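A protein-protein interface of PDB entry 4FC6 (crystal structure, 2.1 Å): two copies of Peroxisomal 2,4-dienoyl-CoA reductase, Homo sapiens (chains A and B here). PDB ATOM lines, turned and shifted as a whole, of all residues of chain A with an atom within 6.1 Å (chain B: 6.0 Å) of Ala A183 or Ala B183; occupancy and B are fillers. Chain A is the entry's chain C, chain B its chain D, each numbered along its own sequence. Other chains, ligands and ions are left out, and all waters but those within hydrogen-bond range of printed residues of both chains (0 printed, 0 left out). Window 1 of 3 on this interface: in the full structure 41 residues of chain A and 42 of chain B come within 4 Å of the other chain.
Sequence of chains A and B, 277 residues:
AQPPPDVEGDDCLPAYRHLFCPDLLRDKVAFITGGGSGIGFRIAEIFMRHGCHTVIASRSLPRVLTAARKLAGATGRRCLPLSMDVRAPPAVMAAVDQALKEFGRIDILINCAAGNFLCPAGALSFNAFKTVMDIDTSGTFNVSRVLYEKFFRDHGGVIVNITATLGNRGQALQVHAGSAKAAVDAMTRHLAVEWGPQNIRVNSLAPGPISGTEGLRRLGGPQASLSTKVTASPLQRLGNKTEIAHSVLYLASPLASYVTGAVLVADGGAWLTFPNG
The backbone carbonyl oxygen of Ala A180 is in hydrogen-bond range of the side-chain hydroxyl of Thr A137, 3.1 Å away. OG of Ser A179 sits at hydrogen-bond distance from O of Val A175 (2.6 Å). The backbone NH (N) of Ala B180 sits at hydrogen-bond distance from the side-chain sulfur (SD) of Met B133 (3.5 Å). The side-chain hydroxyl (OG1) of Thr B137 sits at hydrogen-bond distance from the backbone carbonyl oxygen (O) of Ala B180, 3.0 Å away.
Of chain B, only Ser B179 (3.2 Å) and Ala B183 (3.9 Å) come within 4 Å of Ala A183. Printed residues of chain A within 4 Å of Ala B183: Ser A179 (3.4 Å) and Ala A183 (3.9 Å). Printed residues of chain B within 4 Å of Thr A137: Met B133. Of the printed residues of chain A, Met B187 touches Val A175 (3.6 Å) and Ser A179 (3.6 Å). Of the printed residues of chain A, Ala B186 touches Gly A178 and Ala A182. The nearest printed residue of chain A that does not touch Ala B183 is Ala A182 (4.6 Å).
Among the printed residues, pairs that only touch across the chains: Ser A179 with Ala B183 (3.4 Å), Ser A179 with Met B187 (3.6 Å), Val A175 with Met B187 (3.6 Å), Met A187 with Ser B179 (3.7 Å), Ala A182 with Ala B186 (3.7 Å), Ala A186 with Ala B182 (3.7 Å), Ala A186 with Gly B178 (3.8 Å), Gly A178 with Ala B186 (3.9 Å), Met A133 with Thr B137 (3.9 Å), Ala A183 with Ala B183 (3.9 Å), Thr A137 with Met B133 (3.9 Å) and Ala A182 with Ala B182 (3.98 Å).
The backbone carbonyl oxygen (O) of Ala A183 is in hydrogen-bond range of the side-chain hydroxyl (OG) of Ser B179.
Printed residues of chain B that touch a printed residue of chain A: Met B133, Thr B137, Gly B178, Ser B179, Ala B182, Ala B183, Ala B186 and Met B187. Printed residues of chain A that touch a printed residue of chain B: Met A133, Thr A137, Val A175, Gly A178, Ser A179, Ala A182, Ala A183, Ala A186 and Met A187.
Met A133 touches Thr B137, and with the chains exchanged Thr A137 touches Met B133. Gly A178 touches Ala B186, and with the chains exchanged Ala A186 touches Gly B178. Ser A179 touches Met B187, and with the chains exchanged Met A187 touches Ser B179. Ala A182 touches its own counterpart, Ala B182. Of the 13 pairs that touch across the chains among the printed residues, 12 have their exchanged pair printed and touching as well.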
ATOM      1  N   MET A 133      17.686   5.505  22.915  1.00  0.00           N
ATOM      2  CA  MET A 133      17.998   4.489  21.900  1.00  0.00           C
ATOM      3  C   MET A 133      19.482   4.561  21.594  1.00  0.00           C
ATOM      4  O   MET A 133      20.140   3.558  21.410  1.00  0.00           O
ATOM      5  CB  MET A 133      17.315   4.792  20.562  1.00  0.00           C
ATOM      6  CG  MET A 133      15.854   4.449  20.438  1.00  0.00           C
ATOM      7  SD  MET A 133      15.510   2.784  20.997  1.00  0.00           S
ATOM      8  CE  MET A 133      15.036   3.283  22.636  1.00  0.00           C
ATOM      9  N   THR A 137      21.184   1.301  23.070  1.00  0.00           N
ATOM     10  CA  THR A 137      21.315   0.402  21.948  1.00  0.00           C
ATOM     11  C   THR A 137      22.500   0.689  21.041  1.00  0.00           C
ATOM     12  O   THR A 137      23.358  -0.190  20.897  1.00  0.00           O
ATOM     13  CB  THR A 137      20.034   0.343  21.118  1.00  0.00           C
ATOM     14  OG1 THR A 137      18.935   0.295  22.027  1.00  0.00           O
ATOM     15  CG2 THR A 137      20.049  -0.911  20.342  1.00  0.00           C
ATOM     16  N   VAL A 175       8.622   3.557  27.779  1.00  0.00           N
ATOM     17  CA  VAL A 175       8.697   3.080  26.384  1.00  0.00           C
ATOM     18  C   VAL A 175      10.134   3.129  25.764  1.00  0.00           C
ATOM     19  O   VAL A 175      10.589   2.141  25.120  1.00  0.00           O
ATOM     20  CB  VAL A 175       7.637   3.800  25.513  1.00  0.00           C
ATOM     21  CG1 VAL A 175       7.947   5.299  25.372  1.00  0.00           C
ATOM     22  CG2 VAL A 175       7.577   3.139  24.164  1.00  0.00           C
ATOM     23  N   GLY A 178      12.568   0.661  27.815  1.00  0.00           N
ATOM     24  CA  GLY A 178      12.138  -0.704  27.618  1.00  0.00           C
ATOM     25  C   GLY A 178      12.385  -1.149  26.170  1.00  0.00           C
ATOM     26  O   GLY A 178      12.738  -2.331  25.938  1.00  0.00           O
ATOM     27  N   SER A 179      12.136  -0.244  25.227  1.00  0.00           N
ATOM     28  CA  SER A 179      12.435  -0.503  23.803  1.00  0.00           C
ATOM     29  C   SER A 179      13.929  -0.654  23.550  1.00  0.00           C
ATOM     30  O   SER A 179      14.375  -1.612  22.891  1.00  0.00           O
ATOM     31  CB  SER A 179      11.912   0.616  22.904  1.00  0.00           C
ATOM     32  OG  SER A 179      10.496   0.657  23.019  1.00  0.00           O
ATOM     33  N   ALA A 180      14.702   0.252  24.114  1.00  0.00           N
ATOM     34  CA  ALA A 180      16.176   0.237  23.966  1.00  0.00           C
ATOM     35  C   ALA A 180      16.753  -1.058  24.543  1.00  0.00           C
ATOM     36  O   ALA A 180      17.611  -1.703  23.926  1.00  0.00           O
ATOM     37  CB  ALA A 180      16.822   1.424  24.701  1.00  0.00           C
ATOM     38  N   LYS A 181      16.343  -1.389  25.776  1.00  0.00           N
ATOM     39  CA  LYS A 181      16.876  -2.593  26.399  1.00  0.00           C
ATOM     40  C   LYS A 181      16.427  -3.906  25.703  1.00  0.00           C
ATOM     41  O   LYS A 181      17.158  -4.869  25.638  1.00  0.00           O
ATOM     42  CB  LYS A 181      16.545  -2.575  27.905  1.00  0.00           C
ATOM     43  CG  LYS A 181      17.241  -1.437  28.647  1.00  0.00           C
ATOM     44  CD  LYS A 181      18.763  -1.628  28.682  1.00  0.00           C
ATOM     45  CE  LYS A 181      19.322  -0.761  29.871  1.00  0.00           C
ATOM     46  NZ  LYS A 181      20.812  -0.948  29.962  1.00  0.00           N
ATOM     47  N   ALA A 182      15.195  -3.979  25.228  1.00  0.00           N
ATOM     48  CA  ALA A 182      14.788  -5.135  24.428  1.00  0.00           C
ATOM     49  C   ALA A 182      15.641  -5.301  23.161  1.00  0.00           C
ATOM     50  O   ALA A 182      15.883  -6.429  22.734  1.00  0.00           O
ATOM     51  CB  ALA A 182      13.295  -5.036  24.059  1.00  0.00           C
ATOM     52  N   ALA A 183      16.022  -4.195  22.503  1.00  0.00           N
ATOM     53  CA  ALA A 183      16.920  -4.280  21.323  1.00  0.00           C
ATOM     54  C   ALA A 183      18.287  -4.893  21.728  1.00  0.00           C
ATOM     55  O   ALA A 183      18.884  -5.727  20.979  1.00  0.00           O
ATOM     56  CB  ALA A 183      17.125  -2.898  20.726  1.00  0.00           C
ATOM     57  N   VAL A 184      18.774  -4.473  22.910  1.00  0.00           N
ATOM     58  CA  VAL A 184      20.054  -4.971  23.368  1.00  0.00           C
ATOM     59  C   VAL A 184      19.994  -6.482  23.625  1.00  0.00           C
ATOM     60  O   VAL A 184      20.940  -7.227  23.317  1.00  0.00           O
ATOM     61  CB  VAL A 184      20.534  -4.194  24.601  1.00  0.00           C
ATOM     62  CG1 VAL A 184      21.827  -4.815  25.139  1.00  0.00           C
ATOM     63  CG2 VAL A 184      20.761  -2.745  24.176  1.00  0.00           C
ATOM     64  N   ASP A 185      18.876  -6.920  24.186  1.00  0.00           N
ATOM     65  CA  ASP A 185      18.664  -8.350  24.389  1.00  0.00           C
ATOM     66  C   ASP A 185      18.705  -9.132  23.086  1.00  0.00           C
ATOM     67  O   ASP A 185      19.332 -10.227  23.055  1.00  0.00           O
ATOM     68  CB  ASP A 185      17.375  -8.653  25.168  1.00  0.00           C
ATOM     69  CG  ASP A 185      17.551  -8.493  26.686  1.00  0.00           C
ATOM     70  OD1 ASP A 185      18.694  -8.466  27.224  1.00  0.00           O
ATOM     71  OD2 ASP A 185      16.523  -8.397  27.382  1.00  0.00           O
ATOM     72  N   ALA A 186      18.075  -8.586  22.024  1.00  0.00           N
ATOM     73  CA  ALA A 186      18.176  -9.212  20.716  1.00  0.00           C
ATOM     74  C   ALA A 186      19.603  -9.169  20.208  1.00  0.00           C
ATOM     75  O   ALA A 186      20.090 -10.159  19.644  1.00  0.00           O
ATOM     76  CB  ALA A 186      17.256  -8.580  19.680  1.00  0.00           C
ATOM     77  N   MET A 187      20.261  -8.028  20.379  1.00  0.00           N
ATOM     78  CA  MET A 187      21.665  -7.893  19.945  1.00  0.00           C
ATOM     79  C   MET A 187      22.531  -8.969  20.589  1.00  0.00           C
ATOM     80  O   MET A 187      23.461  -9.450  19.941  1.00  0.00           O
ATOM     81  CB  MET A 187      22.227  -6.513  20.275  1.00  0.00           C
ATOM     82  CG  MET A 187      23.557  -6.128  19.617  1.00  0.00           C
ATOM     83  SD  MET A 187      24.206  -4.649  20.424  1.00  0.00           S
ATOM     84  CE  MET A 187      22.844  -3.492  20.244  1.00  0.00           C
ATOM     85  N   THR A 188      22.266  -9.309  21.856  1.00  0.00           N
ATOM     86  CA  THR A 188      22.988 -10.388  22.567  1.00  0.00           C
ATOM     87  C   THR A 188      22.956 -11.719  21.771  1.00  0.00           C
ATOM     88  O   THR A 188      23.991 -12.345  21.508  1.00  0.00           O
ATOM     89  CB  THR A 188      22.443 -10.592  24.012  1.00  0.00           C
ATOM     90  OG1 THR A 188      22.895  -9.505  24.815  1.00  0.00           O
ATOM     91  CG2 THR A 188      22.904 -11.853  24.631  1.00  0.00           C
ATOM     92  N   MET B 133      18.053   1.546  13.242  1.00  0.00           N
ATOM     93  CA  MET B 133      17.352   1.823  14.476  1.00  0.00           C
ATOM     94  C   MET B 133      16.525   3.107  14.334  1.00  0.00           C
ATOM     95  O   MET B 133      15.393   3.182  14.867  1.00  0.00           O
ATOM     96  CB  MET B 133      18.342   1.902  15.668  1.00  0.00           C
ATOM     97  CG  MET B 133      19.231   0.661  15.837  1.00  0.00           C
ATOM     98  SD  MET B 133      18.339  -0.820  16.416  1.00  0.00           S
ATOM     99  CE  MET B 133      17.250  -0.109  17.680  1.00  0.00           C
ATOM    100  N   THR B 137      12.799   1.998  14.510  1.00  0.00           N
ATOM    101  CA  THR B 137      12.380   2.141  15.889  1.00  0.00           C
ATOM    102  C   THR B 137      11.944   3.562  16.179  1.00  0.00           C
ATOM    103  O   THR B 137      10.763   3.798  16.558  1.00  0.00           O
ATOM    104  CB  THR B 137      13.461   1.673  16.921  1.00  0.00           C
ATOM    105  OG1 THR B 137      13.978   0.388  16.563  1.00  0.00           O
ATOM    106  CG2 THR B 137      12.863   1.592  18.336  1.00  0.00           C
ATOM    107  N   GLY B 178      17.172  -7.072  13.458  1.00  0.00           N
ATOM    108  CA  GLY B 178      16.613  -7.833  14.555  1.00  0.00           C
ATOM    109  C   GLY B 178      16.508  -6.995  15.828  1.00  0.00           C
ATOM    110  O   GLY B 178      15.584  -7.132  16.606  1.00  0.00           O
ATOM    111  N   SER B 179      17.516  -6.202  16.101  1.00  0.00           N
ATOM    112  CA  SER B 179      17.501  -5.339  17.269  1.00  0.00           C
ATOM    113  C   SER B 179      16.390  -4.304  17.200  1.00  0.00           C
ATOM    114  O   SER B 179      15.705  -4.145  18.163  1.00  0.00           O
ATOM    115  CB  SER B 179      18.812  -4.591  17.423  1.00  0.00           C
ATOM    116  OG  SER B 179      19.878  -5.508  17.631  1.00  0.00           O
ATOM    117  N   ALA B 180      16.269  -3.606  16.070  1.00  0.00           N
ATOM    118  CA  ALA B 180      15.285  -2.539  15.857  1.00  0.00           C
ATOM    119  C   ALA B 180      13.880  -3.095  15.920  1.00  0.00           C
ATOM    120  O   ALA B 180      12.967  -2.486  16.515  1.00  0.00           O
ATOM    121  CB  ALA B 180      15.538  -1.856  14.500  1.00  0.00           C
ATOM    122  N   LYS B 181      13.689  -4.254  15.315  1.00  0.00           N
ATOM    123  CA  LYS B 181      12.356  -4.855  15.289  1.00  0.00           C
ATOM    124  C   LYS B 181      11.956  -5.410  16.682  1.00  0.00           C
ATOM    125  O   LYS B 181      10.787  -5.324  17.070  1.00  0.00           O
ATOM    126  CB  LYS B 181      12.216  -5.938  14.202  1.00  0.00           C
ATOM    127  CG  LYS B 181      12.284  -5.445  12.728  1.00  0.00           C
ATOM    128  CD  LYS B 181      11.257  -4.331  12.394  1.00  0.00           C
ATOM    129  CE  LYS B 181      10.965  -4.328  10.887  1.00  0.00           C
ATOM    130  NZ  LYS B 181       9.804  -3.497  10.458  1.00  0.00           N
ATOM    131  N   ALA B 182      12.933  -5.966  17.422  1.00  0.00           N
ATOM    132  CA  ALA B 182      12.638  -6.381  18.798  1.00  0.00           C
ATOM    133  C   ALA B 182      12.284  -5.155  19.644  1.00  0.00           C
ATOM    134  O   ALA B 182      11.414  -5.246  20.512  1.00  0.00           O
ATOM    135  CB  ALA B 182      13.822  -7.117  19.396  1.00  0.00           C
ATOM    136  N   ALA B 183      12.974  -4.030  19.418  1.00  0.00           N
ATOM    137  CA  ALA B 183      12.596  -2.782  20.068  1.00  0.00           C
ATOM    138  C   ALA B 183      11.111  -2.396  19.747  1.00  0.00           C
ATOM    139  O   ALA B 183      10.388  -1.942  20.624  1.00  0.00           O
ATOM    140  CB  ALA B 183      13.541  -1.663  19.637  1.00  0.00           C
ATOM    141  N   VAL B 184      10.697  -2.533  18.497  1.00  0.00           N
ATOM    142  CA  VAL B 184       9.323  -2.162  18.110  1.00  0.00           C
ATOM    143  C   VAL B 184       8.311  -3.105  18.779  1.00  0.00           C
ATOM    144  O   VAL B 184       7.240  -2.659  19.228  1.00  0.00           O
ATOM    145  CB  VAL B 184       9.165  -2.100  16.588  1.00  0.00           C
ATOM    146  CG1 VAL B 184       7.678  -1.973  16.183  1.00  0.00           C
ATOM    147  CG2 VAL B 184       9.968  -0.890  16.063  1.00  0.00           C
ATOM    148  N   ASP B 185       8.651  -4.385  18.923  1.00  0.00           N
ATOM    149  CA  ASP B 185       7.702  -5.305  19.627  1.00  0.00           C
ATOM    150  C   ASP B 185       7.494  -4.933  21.094  1.00  0.00           C
ATOM    151  O   ASP B 185       6.359  -4.946  21.616  1.00  0.00           O
ATOM    152  CB  ASP B 185       8.162  -6.753  19.536  1.00  0.00           C
ATOM    153  CG  ASP B 185       7.877  -7.404  18.179  1.00  0.00           C
ATOM    154  OD1 ASP B 185       6.917  -7.021  17.396  1.00  0.00           O
ATOM    155  OD2 ASP B 185       8.610  -8.400  17.924  1.00  0.00           O
ATOM    156  N   ALA B 186       8.577  -4.574  21.778  1.00  0.00           N
ATOM    157  CA  ALA B 186       8.462  -4.039  23.143  1.00  0.00           C
ATOM    158  C   ALA B 186       7.655  -2.733  23.099  1.00  0.00           C
ATOM    159  O   ALA B 186       6.767  -2.491  23.942  1.00  0.00           O
ATOM    160  CB  ALA B 186       9.855  -3.761  23.732  1.00  0.00           C
ATOM    161  N   MET B 187       7.966  -1.886  22.132  1.00  0.00           N
ATOM    162  CA  MET B 187       7.226  -0.622  22.014  1.00  0.00           C
ATOM    163  C   MET B 187       5.719  -0.869  21.916  1.00  0.00           C
ATOM    164  O   MET B 187       4.923  -0.094  22.454  1.00  0.00           O
ATOM    165  CB  MET B 187       7.692   0.226  20.813  1.00  0.00           C
ATOM    166  CG  MET B 187       7.165   1.662  20.854  1.00  0.00           C
ATOM    167  SD  MET B 187       7.336   2.484  19.255  1.00  0.00           S
ATOM    168  CE  MET B 187       9.106   2.334  18.926  1.00  0.00           C
ATOM    169  N   THR B 188       5.342  -1.939  21.233  1.00  0.00           N
ATOM    170  CA  THR B 188       3.947  -2.356  21.094  1.00  0.00           C
ATOM    171  C   THR B 188       3.293  -2.592  22.433  1.00  0.00           C
ATOM    172  O   THR B 188       2.169  -2.119  22.678  1.00  0.00           O
ATOM    173  CB  THR B 188       3.872  -3.636  20.207  1.00  0.00           C
ATOM    174  OG1 THR B 188       4.097  -3.245  18.871  1.00  0.00           O
ATOM    175  CG2 THR B 188       2.470  -4.303  20.290  1.00  0.00           C
